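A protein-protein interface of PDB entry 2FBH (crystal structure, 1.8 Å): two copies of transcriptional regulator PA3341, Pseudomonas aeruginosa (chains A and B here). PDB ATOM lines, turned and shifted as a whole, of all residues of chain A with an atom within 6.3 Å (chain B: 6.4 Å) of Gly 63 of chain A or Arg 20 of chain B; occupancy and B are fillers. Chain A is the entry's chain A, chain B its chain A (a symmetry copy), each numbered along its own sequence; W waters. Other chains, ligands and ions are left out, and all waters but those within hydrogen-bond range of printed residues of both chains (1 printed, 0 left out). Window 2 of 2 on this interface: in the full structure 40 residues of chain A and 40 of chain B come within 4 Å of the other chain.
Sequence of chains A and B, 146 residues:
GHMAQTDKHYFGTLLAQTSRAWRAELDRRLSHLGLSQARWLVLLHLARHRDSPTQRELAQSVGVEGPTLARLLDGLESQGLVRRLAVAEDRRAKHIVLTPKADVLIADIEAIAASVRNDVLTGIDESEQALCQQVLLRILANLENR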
ATOM      1  N   SER A  19      20.915   3.369 -11.537  1.00  0.00           N
ATOM      2  CA  SER A  19      20.968   3.876 -10.164  1.00  0.00           C
ATOM      3  C   SER A  19      20.508   5.352 -10.111  1.00  0.00           C
ATOM      4  O   SER A  19      19.706   5.677  -9.253  1.00  0.00           O
ATOM      5  CB  SER A  19      22.326   3.674  -9.545  1.00  0.00           C
ATOM      6  OG  SER A  19      22.152   3.945  -8.103  1.00  0.00           O
ATOM      7  N   LEU A  41      17.958  10.485   2.297  1.00  0.00           N
ATOM      8  CA  LEU A  41      18.781   9.271   2.123  1.00  0.00           C
ATOM      9  C   LEU A  41      19.641   8.948   3.370  1.00  0.00           C
ATOM     10  O   LEU A  41      19.913   7.805   3.666  1.00  0.00           O
ATOM     11  CB  LEU A  41      19.647   9.438   0.883  1.00  0.00           C
ATOM     12  CG  LEU A  41      20.139   8.244   0.064  1.00  0.00           C
ATOM     13  CD1 LEU A  41      21.541   7.885   0.473  1.00  0.00           C
ATOM     14  CD2 LEU A  41      19.212   7.024   0.172  1.00  0.00           C
ATOM     15  N   HIS A  45      18.830   5.636   5.610  1.00  0.00           N
ATOM     16  CA  HIS A  45      19.875   4.763   6.092  1.00  0.00           C
ATOM     17  C   HIS A  45      19.897   4.622   7.621  1.00  0.00           C
ATOM     18  O   HIS A  45      20.155   3.537   8.162  1.00  0.00           O
ATOM     19  CB  HIS A  45      21.198   5.210   5.531  1.00  0.00           C
ATOM     20  CG  HIS A  45      21.360   4.873   4.065  1.00  0.00           C
ATOM     21  ND1 HIS A  45      22.384   4.075   3.590  1.00  0.00           N
ATOM     22  CD2 HIS A  45      20.597   5.181   2.985  1.00  0.00           C
ATOM     23  CE1 HIS A  45      22.280   3.959   2.271  1.00  0.00           C
ATOM     24  NE2 HIS A  45      21.203   4.620   1.880  1.00  0.00           N
ATOM     25  N   LEU A  58      28.116   6.568   8.570  1.00  0.00           N
ATOM     26  CA  LEU A  58      26.959   7.046   7.824  1.00  0.00           C
ATOM     27  C   LEU A  58      27.374   7.629   6.466  1.00  0.00           C
ATOM     28  O   LEU A  58      26.674   7.457   5.477  1.00  0.00           O
ATOM     29  CB  LEU A  58      26.246   8.107   8.674  1.00  0.00           C
ATOM     30  CG  LEU A  58      24.850   8.558   8.286  1.00  0.00           C
ATOM     31  CD1 LEU A  58      23.831   7.410   7.973  1.00  0.00           C
ATOM     32  CD2 LEU A  58      24.328   9.462   9.459  1.00  0.00           C
ATOM     33  N   ALA A  59      28.516   8.295   6.437  1.00  0.00           N
ATOM     34  CA  ALA A  59      29.030   8.921   5.235  1.00  0.00           C
ATOM     35  C   ALA A  59      29.356   7.809   4.219  1.00  0.00           C
ATOM     36  O   ALA A  59      28.897   7.846   3.069  1.00  0.00           O
ATOM     37  CB  ALA A  59      30.268   9.719   5.580  1.00  0.00           C
ATOM     38  N   GLN A  60      30.108   6.807   4.682  1.00  0.00           N
ATOM     39  CA  GLN A  60      30.368   5.578   3.924  1.00  0.00           C
ATOM     40  C   GLN A  60      29.109   5.078   3.237  1.00  0.00           C
ATOM     41  O   GLN A  60      29.064   5.015   2.001  1.00  0.00           O
ATOM     42  CB  GLN A  60      31.015   4.493   4.806  1.00  0.00           C
ATOM     43  CG  GLN A  60      32.526   4.684   4.968  1.00  0.00           C
ATOM     44  CD  GLN A  60      33.196   3.787   6.029  1.00  0.00           C
ATOM     45  OE1 GLN A  60      32.542   2.969   6.726  1.00  0.00           O
ATOM     46  NE2 GLN A  60      34.522   3.953   6.167  1.00  0.00           N
ATOM     47  N   SER A  61      28.067   4.786   4.007  1.00  0.00           N
ATOM     48  CA  SER A  61      26.913   4.099   3.445  1.00  0.00           C
ATOM     49  C   SER A  61      25.969   4.964   2.619  1.00  0.00           C
ATOM     50  O   SER A  61      25.341   4.458   1.684  1.00  0.00           O
ATOM     51  CB  SER A  61      26.161   3.287   4.519  1.00  0.00           C
ATOM     52  OG  SER A  61      25.042   3.934   5.079  1.00  0.00           O
ATOM     53  N   VAL A  62      25.849   6.241   2.985  1.00  0.00           N
ATOM     54  CA  VAL A  62      25.000   7.195   2.277  1.00  0.00           C
ATOM     55  C   VAL A  62      25.653   7.612   0.956  1.00  0.00           C
ATOM     56  O   VAL A  62      24.963   7.966  -0.027  1.00  0.00           O
ATOM     57  CB  VAL A  62      24.775   8.432   3.142  1.00  0.00           C
ATOM     58  CG1 VAL A  62      24.393   9.616   2.283  1.00  0.00           C
ATOM     59  CG2 VAL A  62      23.719   8.135   4.191  1.00  0.00           C
ATOM     60  N   GLY A  63      26.985   7.661   1.009  1.00  0.00           N
ATOM     61  CA  GLY A  63      27.867   7.705  -0.140  1.00  0.00           C
ATOM     62  C   GLY A  63      28.474   9.058  -0.402  1.00  0.00           C
ATOM     63  O   GLY A  63      28.607   9.463  -1.550  1.00  0.00           O
ATOM     64  N   VAL A  64      28.841   9.757   0.668  1.00  0.00           N
ATOM     65  CA  VAL A  64      29.112  11.182   0.598  1.00  0.00           C
ATOM     66  C   VAL A  64      30.320  11.381   1.479  1.00  0.00           C
ATOM     67  O   VAL A  64      30.541  10.586   2.418  1.00  0.00           O
ATOM     68  CB  VAL A  64      27.861  11.945   1.122  1.00  0.00           C
ATOM     69  CG1 VAL A  64      28.001  12.298   2.587  1.00  0.00           C
ATOM     70  CG2 VAL A  64      27.517  13.161   0.274  1.00  0.00           C
ATOM     71  N   GLU A  65      31.109  12.420   1.178  1.00  0.00           N
ATOM     72  CA  GLU A  65      32.261  12.843   1.995  1.00  0.00           C
ATOM     73  C   GLU A  65      31.772  13.314   3.363  1.00  0.00           C
ATOM     74  O   GLU A  65      30.643  13.792   3.475  1.00  0.00           O
ATOM     75  CB  GLU A  65      32.992  13.998   1.301  1.00  0.00           C
ATOM     76  CG  GLU A  65      34.420  14.300   1.785  1.00  0.00           C
ATOM     77  CD  GLU A  65      34.960  15.613   1.213  1.00  0.00           C
ATOM     78  OE1 GLU A  65      34.143  16.390   0.683  1.00  0.00           O
ATOM     79  OE2 GLU A  65      36.185  15.877   1.301  1.00  0.00           O
ATOM     80  N   LEU B  15      22.347  -1.544  -5.666  1.00  0.00           N
ATOM     81  CA  LEU B  15      22.723  -0.985  -6.948  1.00  0.00           C
ATOM     82  C   LEU B  15      23.503   0.327  -6.772  1.00  0.00           C
ATOM     83  O   LEU B  15      24.530   0.546  -7.391  1.00  0.00           O
ATOM     84  CB  LEU B  15      21.431  -0.754  -7.792  1.00  0.00           C
ATOM     85  CG  LEU B  15      21.520   0.031  -9.047  1.00  0.00           C
ATOM     86  CD1 LEU B  15      22.477  -0.740  -9.941  1.00  0.00           C
ATOM     87  CD2 LEU B  15      20.103   0.000  -9.681  1.00  0.00           C
ATOM     88  N   ALA B  16      23.010   1.171  -5.855  1.00  0.00           N
ATOM     89  CA  ALA B  16      23.683   2.491  -5.687  1.00  0.00           C
ATOM     90  C   ALA B  16      25.069   2.319  -5.118  1.00  0.00           C
ATOM     91  O   ALA B  16      26.039   3.058  -5.482  1.00  0.00           O
ATOM     92  CB  ALA B  16      22.842   3.310  -4.774  1.00  0.00           C
ATOM     93  N   GLN B  17      25.186   1.416  -4.153  1.00  0.00           N
ATOM     94  CA  GLN B  17      26.494   1.160  -3.522  1.00  0.00           C
ATOM     95  C   GLN B  17      27.537   0.593  -4.496  1.00  0.00           C
ATOM     96  O   GLN B  17      28.725   0.986  -4.429  1.00  0.00           O
ATOM     97  CB  GLN B  17      26.303   0.229  -2.342  1.00  0.00           C
ATOM     98  CG  GLN B  17      25.610   0.945  -1.145  1.00  0.00           C
ATOM     99  CD  GLN B  17      25.529   0.011   0.095  1.00  0.00           C
ATOM    100  OE1 GLN B  17      25.974  -1.150   0.052  1.00  0.00           O
ATOM    101  NE2 GLN B  17      25.012   0.565   1.239  1.00  0.00           N
ATOM    102  N   THR B  18      27.092  -0.314  -5.375  1.00  0.00           N
ATOM    103  CA  THR B  18      27.970  -0.942  -6.344  1.00  0.00           C
ATOM    104  C   THR B  18      28.412   0.120  -7.353  1.00  0.00           C
ATOM    105  O   THR B  18      29.576   0.210  -7.681  1.00  0.00           O
ATOM    106  CB  THR B  18      27.235  -2.091  -7.078  1.00  0.00           C
ATOM    107  OG1 THR B  18      26.753  -3.055  -6.128  1.00  0.00           O
ATOM    108  CG2 THR B  18      28.238  -2.801  -7.996  1.00  0.00           C
ATOM    109  N   SER B  19      27.451   0.924  -7.827  1.00  0.00           N
ATOM    110  CA  SER B  19      27.739   2.037  -8.733  1.00  0.00           C
ATOM    111  C   SER B  19      28.720   3.035  -8.073  1.00  0.00           C
ATOM    112  O   SER B  19      29.673   3.425  -8.725  1.00  0.00           O
ATOM    113  CB  SER B  19      26.479   2.705  -9.217  1.00  0.00           C
ATOM    114  OG  SER B  19      26.896   3.588 -10.327  1.00  0.00           O
ATOM    115  N   ARG B  20      28.459   3.456  -6.838  1.00  0.00           N
ATOM    116  CA  ARG B  20      29.374   4.366  -6.124  1.00  0.00           C
ATOM    117  C   ARG B  20      30.752   3.768  -6.011  1.00  0.00           C
ATOM    118  O   ARG B  20      31.749   4.516  -6.166  1.00  0.00           O
ATOM    119  CB  ARG B  20      28.856   4.644  -4.739  1.00  0.00           C
ATOM    120  CG  ARG B  20      29.714   5.569  -3.867  1.00  0.00           C
ATOM    121  CD  ARG B  20      28.903   5.870  -2.573  1.00  0.00           C
ATOM    122  NE  ARG B  20      27.442   5.912  -2.820  1.00  0.00           N
ATOM    123  CZ  ARG B  20      26.803   6.810  -3.593  1.00  0.00           C
ATOM    124  NH1 ARG B  20      27.476   7.805  -4.184  1.00  0.00           N
ATOM    125  NH2 ARG B  20      25.477   6.735  -3.756  1.00  0.00           N
ATOM    126  N   ALA B  21      30.829   2.483  -5.702  1.00  0.00           N
ATOM    127  CA  ALA B  21      32.170   1.834  -5.502  1.00  0.00           C
ATOM    128  C   ALA B  21      32.914   1.844  -6.842  1.00  0.00           C
ATOM    129  O   ALA B  21      34.128   2.099  -6.887  1.00  0.00           O
ATOM    130  CB  ALA B  21      31.968   0.394  -4.980  1.00  0.00           C
ATOM    131  N   TRP B  22      32.217   1.561  -7.948  1.00  0.00           N
ATOM    132  CA  TRP B  22      32.886   1.487  -9.240  1.00  0.00           C
ATOM    133  C   TRP B  22      33.355   2.904  -9.647  1.00  0.00           C
ATOM    134  O   TRP B  22      34.521   3.116 -10.034  1.00  0.00           O
ATOM    135  CB  TRP B  22      31.898   0.933 -10.260  1.00  0.00           C
ATOM    136  CG  TRP B  22      32.419   0.632 -11.589  1.00  0.00           C
ATOM    137  CD1 TRP B  22      33.392   1.290 -12.289  1.00  0.00           C
ATOM    138  CD2 TRP B  22      31.909  -0.367 -12.436  1.00  0.00           C
ATOM    139  NE1 TRP B  22      33.535   0.749 -13.565  1.00  0.00           N
ATOM    140  CE2 TRP B  22      32.640  -0.291 -13.661  1.00  0.00           C
ATOM    141  CE3 TRP B  22      30.895  -1.327 -12.281  1.00  0.00           C
ATOM    142  CZ2 TRP B  22      32.442  -1.162 -14.711  1.00  0.00           C
ATOM    143  CZ3 TRP B  22      30.666  -2.223 -13.394  1.00  0.00           C
ATOM    144  CH2 TRP B  22      31.431  -2.113 -14.572  1.00  0.00           C
ATOM    145  N   ARG B  23      32.482   3.888  -9.519  1.00  0.00           N
ATOM    146  CA  ARG B  23      32.930   5.270  -9.818  1.00  0.00           C
ATOM    147  C   ARG B  23      34.061   5.767  -8.880  1.00  0.00           C
ATOM    148  O   ARG B  23      34.925   6.536  -9.318  1.00  0.00           O
ATOM    149  CB  ARG B  23      31.723   6.187  -9.843  1.00  0.00           C
ATOM    150  CG  ARG B  23      30.653   5.742 -10.873  1.00  0.00           C
ATOM    151  CD  ARG B  23      31.236   5.635 -12.282  1.00  0.00           C
ATOM    152  NE  ARG B  23      30.649   4.547 -13.024  1.00  0.00           N
ATOM    153  CZ  ARG B  23      31.043   4.204 -14.252  1.00  0.00           C
ATOM    154  NH1 ARG B  23      30.459   3.217 -14.868  1.00  0.00           N
ATOM    155  NH2 ARG B  23      32.016   4.860 -14.872  1.00  0.00           N
ATOM    156  N   ALA B  24      34.095   5.302  -7.642  1.00  0.00           N
ATOM    157  CA  ALA B  24      35.206   5.670  -6.704  1.00  0.00           C
ATOM    158  C   ALA B  24      36.485   5.092  -7.233  1.00  0.00           C
ATOM    159  O   ALA B  24      37.554   5.724  -7.179  1.00  0.00           O
ATOM    160  CB  ALA B  24      34.963   5.170  -5.321  1.00  0.00           C
ATOM    161  N   GLU B  25      36.398   3.840  -7.685  1.00  0.00           N
ATOM    162  CA  GLU B  25      37.606   3.164  -8.181  1.00  0.00           C
ATOM    163  C   GLU B  25      38.135   3.841  -9.475  1.00  0.00           C
ATOM    164  O   GLU B  25      39.324   4.060  -9.654  1.00  0.00           O
ATOM    165  CB  GLU B  25      37.335   1.657  -8.453  1.00  0.00           C
ATOM    166  CG  GLU B  25      38.597   0.928  -8.982  1.00  0.00           C
ATOM    167  CD  GLU B  25      39.793   0.874  -7.947  1.00  0.00           C
ATOM    168  OE1 GLU B  25      39.599   1.062  -6.710  1.00  0.00           O
ATOM    169  OE2 GLU B  25      40.944   0.627  -8.431  1.00  0.00           O
HETATM  170  O   HOH W   1      27.932   3.760  -0.663  1.00  0.00           O
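The backbone carbonyl oxygen of Gly 63 of chain A is in hydrogen-bond range of the guanidinium group of Arg 20 of chain B.
The side-chain hydroxyl (OG) of Ser 61 of chain A is in hydrogen-bond range of a ring nitrogen (ND1) of His 45 of chain A (3.0 Å).
Among the printed residues, pairs that only touch across the chains: Ser 19 of chain A with Ala 16 of chain B (3.2 Å), Ser 19 of chain A with Leu 15 of chain B (3.8 Å), Ser 61 of chain A with Gln 17 of chain B (3.9 Å) and Val 62 of chain A with Arg 20 of chain B (3.96 Å).
Of chain B, only Arg 20 comes within 4 Å of Gly 63 of chain A. Printed residues of chain A within 4 Å of Arg 20 of chain B: Val 62 (3.96 Å) and Gly 63 (3.2 Å). Printed residues of chain B within 4 Å of Ser 61 of chain A: Gln 17 (3.9 Å). Printed residues of chain B within 4 Å of Val 62 of chain A: Arg 20. Printed residues of chain A within 4 Å of Ala 16 of chain B: Ser 19. Of the printed residues of chain A, Leu 15 of chain B touches Ser 19 (3.8 Å). Printed residues of chain A within 4 Å of Gln 17 of chain B: Ser 61. The nearest printed residue of chain B that does not touch Gly 63 of chain A is Gln 17 of chain B (7.2 Å). The nearest printed residue of chain B that does not touch Ser 61 of chain A is Arg 20 of chain B (5.2 Å).
Of the 11 printed residues of chain A, 4 touch a printed residue of chain B. Along chain B the printed residues that touch a printed residue of chain A span positions 15 to 20. Among the printed residues, 5 pairs touch across the chains. Among the printed residues, no Asp or Glu carboxylate lies within 4 Å of a Lys or Arg side-chain nitrogen of the other chain.
Position printed for both chains: 19. Of the 5 pairs that touch across the chains among the printed residues, none has its exchanged pair printed and touching as well.
Water W1 lies within hydrogen-bond range of NE of Arg 20 of chain B (3.1 Å) and O of Gln 60 of chain A (3.2 Å).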
